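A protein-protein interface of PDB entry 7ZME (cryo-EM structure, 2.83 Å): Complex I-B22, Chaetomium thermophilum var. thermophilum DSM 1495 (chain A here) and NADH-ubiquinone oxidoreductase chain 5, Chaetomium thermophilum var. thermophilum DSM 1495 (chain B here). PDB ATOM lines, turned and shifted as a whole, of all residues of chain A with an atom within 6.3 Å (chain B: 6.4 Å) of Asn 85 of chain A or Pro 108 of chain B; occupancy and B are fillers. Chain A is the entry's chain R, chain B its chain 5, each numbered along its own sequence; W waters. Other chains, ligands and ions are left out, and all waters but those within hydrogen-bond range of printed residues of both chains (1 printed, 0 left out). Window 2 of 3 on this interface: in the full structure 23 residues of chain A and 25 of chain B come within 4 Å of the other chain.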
ATOM      1  N   LYS A  81      -1.153  35.311  18.456  1.00  0.00           N
ATOM      2  CA  LYS A  81      -0.814  34.091  17.740  1.00  0.00           C
ATOM      3  C   LYS A  81      -0.330  32.981  18.669  1.00  0.00           C
ATOM      4  O   LYS A  81       0.070  31.915  18.196  1.00  0.00           O
ATOM      5  CB  LYS A  81       0.251  34.409  16.681  1.00  0.00           C
ATOM      6  CG  LYS A  81       0.527  33.323  15.664  1.00  0.00           C
ATOM      7  CD  LYS A  81       1.821  33.584  14.933  1.00  0.00           C
ATOM      8  CE  LYS A  81       1.585  33.873  13.472  1.00  0.00           C
ATOM      9  NZ  LYS A  81       2.821  33.687  12.666  1.00  0.00           N
ATOM     10  N   TYR A  82      -0.385  33.196  19.979  1.00  0.00           N
ATOM     11  CA  TYR A  82       0.250  32.291  20.925  1.00  0.00           C
ATOM     12  C   TYR A  82      -0.596  31.037  21.124  1.00  0.00           C
ATOM     13  O   TYR A  82      -1.809  31.116  21.328  1.00  0.00           O
ATOM     14  CB  TYR A  82       0.465  33.027  22.247  1.00  0.00           C
ATOM     15  CG  TYR A  82       0.711  32.164  23.455  1.00  0.00           C
ATOM     16  CD1 TYR A  82       1.823  31.337  23.522  1.00  0.00           C
ATOM     17  CD2 TYR A  82      -0.142  32.201  24.543  1.00  0.00           C
ATOM     18  CE1 TYR A  82       2.068  30.563  24.626  1.00  0.00           C
ATOM     19  CE2 TYR A  82       0.095  31.425  25.651  1.00  0.00           C
ATOM     20  CZ  TYR A  82       1.200  30.608  25.688  1.00  0.00           C
ATOM     21  OH  TYR A  82       1.435  29.829  26.795  1.00  0.00           O
ATOM     22  N   GLU A  83       0.054  29.873  21.054  1.00  0.00           N
ATOM     23  CA  GLU A  83      -0.595  28.562  21.183  1.00  0.00           C
ATOM     24  C   GLU A  83      -1.559  28.290  20.032  1.00  0.00           C
ATOM     25  O   GLU A  83      -2.545  27.568  20.175  1.00  0.00           O
ATOM     26  CB  GLU A  83      -1.324  28.426  22.520  1.00  0.00           C
ATOM     27  CG  GLU A  83      -0.443  28.395  23.738  1.00  0.00           C
ATOM     28  CD  GLU A  83      -1.240  28.285  25.025  1.00  0.00           C
ATOM     29  OE1 GLU A  83      -2.484  28.360  24.968  1.00  0.00           O
ATOM     30  OE2 GLU A  83      -0.620  28.141  26.098  1.00  0.00           O
ATOM     31  N   ARG A  84      -1.260  28.860  18.865  1.00  0.00           N
ATOM     32  CA  ARG A  84      -2.237  28.816  17.783  1.00  0.00           C
ATOM     33  C   ARG A  84      -2.290  27.445  17.120  1.00  0.00           C
ATOM     34  O   ARG A  84      -3.352  26.816  17.065  1.00  0.00           O
ATOM     35  CB  ARG A  84      -1.941  29.898  16.747  1.00  0.00           C
ATOM     36  CG  ARG A  84      -2.717  29.713  15.460  1.00  0.00           C
ATOM     37  CD  ARG A  84      -2.459  30.833  14.485  1.00  0.00           C
ATOM     38  NE  ARG A  84      -2.970  32.100  14.997  1.00  0.00           N
ATOM     39  CZ  ARG A  84      -3.059  33.213  14.282  1.00  0.00           C
ATOM     40  NH1 ARG A  84      -2.677  33.217  13.017  1.00  0.00           N
ATOM     41  NH2 ARG A  84      -3.534  34.318  14.832  1.00  0.00           N
ATOM     42  N   ASN A  85      -1.158  26.960  16.620  1.00  0.00           N
ATOM     43  CA  ASN A  85      -1.137  25.678  15.928  1.00  0.00           C
ATOM     44  C   ASN A  85      -0.196  24.709  16.628  1.00  0.00           C
ATOM     45  O   ASN A  85       0.662  24.098  15.984  1.00  0.00           O
ATOM     46  CB  ASN A  85      -0.745  25.861  14.465  1.00  0.00           C
ATOM     47  CG  ASN A  85      -1.942  26.135  13.573  1.00  0.00           C
ATOM     48  OD1 ASN A  85      -2.065  27.211  12.989  1.00  0.00           O
ATOM     49  ND2 ASN A  85      -2.838  25.163  13.475  1.00  0.00           N
ATOM     50  N   LEU A  86      -0.342  24.585  17.947  1.00  0.00           N
ATOM     51  CA  LEU A  86       0.567  23.788  18.755  1.00  0.00           C
ATOM     52  C   LEU A  86       0.672  22.366  18.208  1.00  0.00           C
ATOM     53  O   LEU A  86      -0.357  21.734  17.936  1.00  0.00           O
ATOM     54  CB  LEU A  86       0.086  23.737  20.204  1.00  0.00           C
ATOM     55  CG  LEU A  86       0.390  24.903  21.138  1.00  0.00           C
ATOM     56  CD1 LEU A  86      -0.430  24.770  22.408  1.00  0.00           C
ATOM     57  CD2 LEU A  86       1.868  24.956  21.458  1.00  0.00           C
ATOM     58  N   PRO A  87       1.881  21.835  18.039  1.00  0.00           N
ATOM     59  CA  PRO A  87       2.025  20.442  17.608  1.00  0.00           C
ATOM     60  C   PRO A  87       1.717  19.475  18.738  1.00  0.00           C
ATOM     61  O   PRO A  87       1.709  19.831  19.917  1.00  0.00           O
ATOM     62  CB  PRO A  87       3.494  20.354  17.191  1.00  0.00           C
ATOM     63  CG  PRO A  87       4.168  21.370  18.047  1.00  0.00           C
ATOM     64  CD  PRO A  87       3.184  22.493  18.233  1.00  0.00           C
ATOM     65  N   VAL B  25      -6.520  19.489  -0.634  1.00  0.00           N
ATOM     66  CA  VAL B  25      -6.671  20.896  -0.273  1.00  0.00           C
ATOM     67  C   VAL B  25      -7.297  21.681  -1.413  1.00  0.00           C
ATOM     68  O   VAL B  25      -8.368  22.279  -1.268  1.00  0.00           O
ATOM     69  CB  VAL B  25      -5.314  21.493   0.137  1.00  0.00           C
ATOM     70  CG1 VAL B  25      -5.511  22.852   0.772  1.00  0.00           C
ATOM     71  CG2 VAL B  25      -4.582  20.553   1.082  1.00  0.00           C
ATOM     72  N   MET B 104      -5.407  31.381   4.368  1.00  0.00           N
ATOM     73  CA  MET B 104      -5.185  30.183   5.159  1.00  0.00           C
ATOM     74  C   MET B 104      -4.326  29.171   4.422  1.00  0.00           C
ATOM     75  O   MET B 104      -4.308  27.993   4.789  1.00  0.00           O
ATOM     76  CB  MET B 104      -6.523  29.570   5.564  1.00  0.00           C
ATOM     77  CG  MET B 104      -7.375  30.496   6.404  1.00  0.00           C
ATOM     78  SD  MET B 104      -6.750  30.626   8.083  1.00  0.00           S
ATOM     79  CE  MET B 104      -7.487  29.178   8.824  1.00  0.00           C
ATOM     80  N   SER B 106      -1.368  28.721   4.618  1.00  0.00           N
ATOM     81  CA  SER B 106      -0.261  28.229   5.479  1.00  0.00           C
ATOM     82  C   SER B 106      -0.793  27.271   6.549  1.00  0.00           C
ATOM     83  O   SER B 106      -0.054  26.349   6.917  1.00  0.00           O
ATOM     84  CB  SER B 106       0.494  29.377   6.089  1.00  0.00           C
ATOM     85  OG  SER B 106       1.586  28.908   6.867  1.00  0.00           O
ATOM     86  N   ASP B 107      -2.029  27.473   7.009  1.00  0.00           N
ATOM     87  CA  ASP B 107      -2.605  26.641   8.101  1.00  0.00           C
ATOM     88  C   ASP B 107      -2.692  25.194   7.634  1.00  0.00           C
ATOM     89  O   ASP B 107      -3.109  24.973   6.489  1.00  0.00           O
ATOM     90  CB  ASP B 107      -3.992  27.143   8.509  1.00  0.00           C
ATOM     91  CG  ASP B 107      -4.606  26.392   9.677  1.00  0.00           C
ATOM     92  OD1 ASP B 107      -5.334  25.414   9.428  1.00  0.00           O
ATOM     93  OD2 ASP B 107      -4.359  26.796  10.825  1.00  0.00           O
ATOM     94  N   PRO B 108      -2.316  24.204   8.467  1.00  0.00           N
ATOM     95  CA  PRO B 108      -2.462  22.826   8.060  1.00  0.00           C
ATOM     96  C   PRO B 108      -3.903  22.349   7.838  1.00  0.00           C
ATOM     97  O   PRO B 108      -4.214  21.952   6.741  1.00  0.00           O
ATOM     98  CB  PRO B 108      -1.928  22.068   9.286  1.00  0.00           C
ATOM     99  CG  PRO B 108      -1.971  23.049  10.432  1.00  0.00           C
ATOM    100  CD  PRO B 108      -1.721  24.389   9.787  1.00  0.00           C
ATOM    101  N   HIS B 109      -4.788  22.579   8.800  1.00  0.00           N
ATOM    102  CA  HIS B 109      -6.160  22.027   8.708  1.00  0.00           C
ATOM    103  C   HIS B 109      -6.946  22.908   7.761  1.00  0.00           C
ATOM    104  O   HIS B 109      -7.728  23.730   8.226  1.00  0.00           O
ATOM    105  CB  HIS B 109      -6.701  21.906  10.124  1.00  0.00           C
ATOM    106  CG  HIS B 109      -5.655  21.420  11.066  1.00  0.00           C
ATOM    107  ND1 HIS B 109      -5.011  20.218  10.883  1.00  0.00           N
ATOM    108  CD2 HIS B 109      -5.118  21.976  12.170  1.00  0.00           C
ATOM    109  CE1 HIS B 109      -4.131  20.048  11.844  1.00  0.00           C
ATOM    110  NE2 HIS B 109      -4.179  21.108  12.649  1.00  0.00           N
ATOM    111  N   ASN B 110      -6.778  22.682   6.468  1.00  0.00           N
ATOM    112  CA  ASN B 110      -7.372  23.615   5.533  1.00  0.00           C
ATOM    113  C   ASN B 110      -8.649  23.059   4.908  1.00  0.00           C
ATOM    114  O   ASN B 110      -9.456  23.831   4.384  1.00  0.00           O
ATOM    115  CB  ASN B 110      -6.316  23.971   4.475  1.00  0.00           C
ATOM    116  CG  ASN B 110      -6.728  25.110   3.571  1.00  0.00           C
ATOM    117  OD1 ASN B 110      -7.816  25.654   3.683  1.00  0.00           O
ATOM    118  ND2 ASN B 110      -5.828  25.501   2.686  1.00  0.00           N
ATOM    119  N   GLN B 111      -8.878  21.744   4.983  1.00  0.00           N
ATOM    120  CA  GLN B 111     -10.163  21.215   4.532  1.00  0.00           C
ATOM    121  C   GLN B 111     -11.263  21.525   5.533  1.00  0.00           C
ATOM    122  O   GLN B 111     -12.385  21.861   5.145  1.00  0.00           O
ATOM    123  CB  GLN B 111     -10.113  19.702   4.324  1.00  0.00           C
ATOM    124  CG  GLN B 111      -9.336  19.238   3.130  1.00  0.00           C
ATOM    125  CD  GLN B 111      -7.868  19.453   3.315  1.00  0.00           C
ATOM    126  OE1 GLN B 111      -7.241  20.172   2.564  1.00  0.00           O
ATOM    127  NE2 GLN B 111      -7.299  18.784   4.305  1.00  0.00           N
ATOM    128  N   PHE B 153     -11.423  27.390  16.017  1.00  0.00           N
ATOM    129  CA  PHE B 153     -10.726  26.638  14.981  1.00  0.00           C
ATOM    130  C   PHE B 153      -9.308  26.296  15.414  1.00  0.00           C
ATOM    131  O   PHE B 153      -8.839  25.170  15.212  1.00  0.00           O
ATOM    132  CB  PHE B 153     -10.713  27.432  13.678  1.00  0.00           C
ATOM    133  CG  PHE B 153     -10.067  26.707  12.535  1.00  0.00           C
ATOM    134  CD1 PHE B 153     -10.668  25.598  11.974  1.00  0.00           C
ATOM    135  CD2 PHE B 153      -8.859  27.138  12.021  1.00  0.00           C
ATOM    136  CE1 PHE B 153     -10.078  24.934  10.929  1.00  0.00           C
ATOM    137  CE2 PHE B 153      -8.268  26.477  10.974  1.00  0.00           C
ATOM    138  CZ  PHE B 153      -8.879  25.372  10.430  1.00  0.00           C
ATOM    139  N   TRP B 154      -8.608  27.258  16.010  1.00  0.00           N
ATOM    140  CA  TRP B 154      -7.306  27.012  16.620  1.00  0.00           C
ATOM    141  C   TRP B 154      -7.557  26.569  18.055  1.00  0.00           C
ATOM    142  O   TRP B 154      -7.402  27.323  19.016  1.00  0.00           O
ATOM    143  CB  TRP B 154      -6.434  28.258  16.540  1.00  0.00           C
ATOM    144  CG  TRP B 154      -6.077  28.618  15.145  1.00  0.00           C
ATOM    145  CD1 TRP B 154      -5.616  27.780  14.181  1.00  0.00           C
ATOM    146  CD2 TRP B 154      -6.172  29.912  14.542  1.00  0.00           C
ATOM    147  NE1 TRP B 154      -5.405  28.470  13.013  1.00  0.00           N
ATOM    148  CE2 TRP B 154      -5.740  29.782  13.209  1.00  0.00           C
ATOM    149  CE3 TRP B 154      -6.580  31.167  14.999  1.00  0.00           C
ATOM    150  CZ2 TRP B 154      -5.702  30.857  12.333  1.00  0.00           C
ATOM    151  CZ3 TRP B 154      -6.541  32.228  14.129  1.00  0.00           C
ATOM    152  CH2 TRP B 154      -6.103  32.069  12.812  1.00  0.00           C
ATOM    153  N   THR B 156      -6.102  24.525  20.062  1.00  0.00           N
ATOM    154  CA  THR B 156      -5.019  24.378  21.023  1.00  0.00           C
ATOM    155  C   THR B 156      -4.720  25.679  21.747  1.00  0.00           C
ATOM    156  O   THR B 156      -3.883  25.693  22.655  1.00  0.00           O
ATOM    157  CB  THR B 156      -3.758  23.861  20.333  1.00  0.00           C
ATOM    158  OG1 THR B 156      -3.281  24.841  19.403  1.00  0.00           O
ATOM    159  CG2 THR B 156      -4.054  22.570  19.602  1.00  0.00           C
ATOM    160  N   ARG B 157      -5.373  26.772  21.343  1.00  0.00           N
ATOM    161  CA  ARG B 157      -5.240  28.080  22.042  1.00  0.00           C
ATOM    162  C   ARG B 157      -6.373  28.199  23.060  1.00  0.00           C
ATOM    163  O   ARG B 157      -7.533  28.152  22.645  1.00  0.00           O
ATOM    164  CB  ARG B 157      -5.317  29.221  21.023  1.00  0.00           C
ATOM    165  CG  ARG B 157      -5.255  30.622  21.609  1.00  0.00           C
ATOM    166  CD  ARG B 157      -5.015  31.631  20.502  1.00  0.00           C
ATOM    167  NE  ARG B 157      -5.371  32.999  20.855  1.00  0.00           N
ATOM    168  CZ  ARG B 157      -4.561  33.864  21.453  1.00  0.00           C
ATOM    169  NH1 ARG B 157      -4.986  35.086  21.722  1.00  0.00           N
ATOM    170  NH2 ARG B 157      -3.334  33.509  21.783  1.00  0.00           N
HETATM  171  O   HOH W   1      -5.132  24.486  16.862  1.00  0.00           O
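The backbone carbonyl oxygen of Arg 84 of chain A sits at hydrogen-bond distance from the side-chain hydroxyl of Thr 156 of chain B (3.1 Å). The side-chain amide oxygen (OD1) of Asn 85 of chain A sits close to the side-chain carboxylate (OD2) of Asp 107 of chain B, 3.2 Å away. The side-chain hydroxyl of Thr 156 of chain B sits at hydrogen-bond distance from the backbone carbonyl oxygen of Glu 83 of chain A (2.9 Å). The backbone NH (N) of Leu 86 of chain A lies within hydrogen-bond range of the side-chain hydroxyl (OG1) of Thr 156 of chain B, at 3.3 Å. The backbone carbonyl oxygen of Tyr 82 of chain A sits at hydrogen-bond distance from the guanidinium group of Arg 157 of chain B, at 2.9 Å. The backbone carbonyl oxygen of Glu 83 of chain A sits at hydrogen-bond distance from the backbone NH of Arg 157 of chain B.
The side-chain carboxylate of Asp 107 of chain B sits at hydrogen-bond distance from the indole nitrogen of Trp 154 of chain B. The side-chain hydroxyl (OH) of Tyr 82 of chain A sits at hydrogen-bond distance from the side-chain carboxylate (OE2) of Glu 83 of chain A. The side-chain carboxylate (OD1) of Asp 107 of chain B is in hydrogen-bond range of the backbone NH (N) of His 109 of chain B, at 3.0 Å.
Among the printed residues, pairs that only touch across the chains: Arg 84 of chain A with Trp 154 of chain B (3.4 Å), Asn 85 of chain A with Pro 108 of chain B (3.8 Å) and Asn 85 of chain A with Trp 154 of chain B (3.6 Å).
Asn 85 of chain A touches three residues of chain B. Of the printed residues of chain A, Pro 108 of chain B touches Asn 85. Of the printed residues of chain A, Thr 156 of chain B touches Glu 83, Arg 84 and Leu 86. Of the printed residues of chain A, Asp 107 of chain B touches Asn 85. Printed residues of chain A within 4 Å of Arg 157 of chain B: Tyr 82 and Glu 83. Of the printed residues of chain B, Leu 86 of chain A touches Thr 156 (3.3 Å). Of the printed residues of chain A, Trp 154 of chain B touches Arg 84 (3.4 Å) and Asn 85 (3.6 Å). The nearest residue of chain B that does not touch Asn 85 of chain A is Thr 156 of chain B (4.1 Å).
Hydrophobic or aromatic side chains of chain A that line the printed part of chain B: Tyr 82 and Leu 86.
Water W1 lies within hydrogen-bond range of O of Arg 84 of chain A (2.9 Å) and OG1 of Thr 156 of chain B (3.2 Å).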
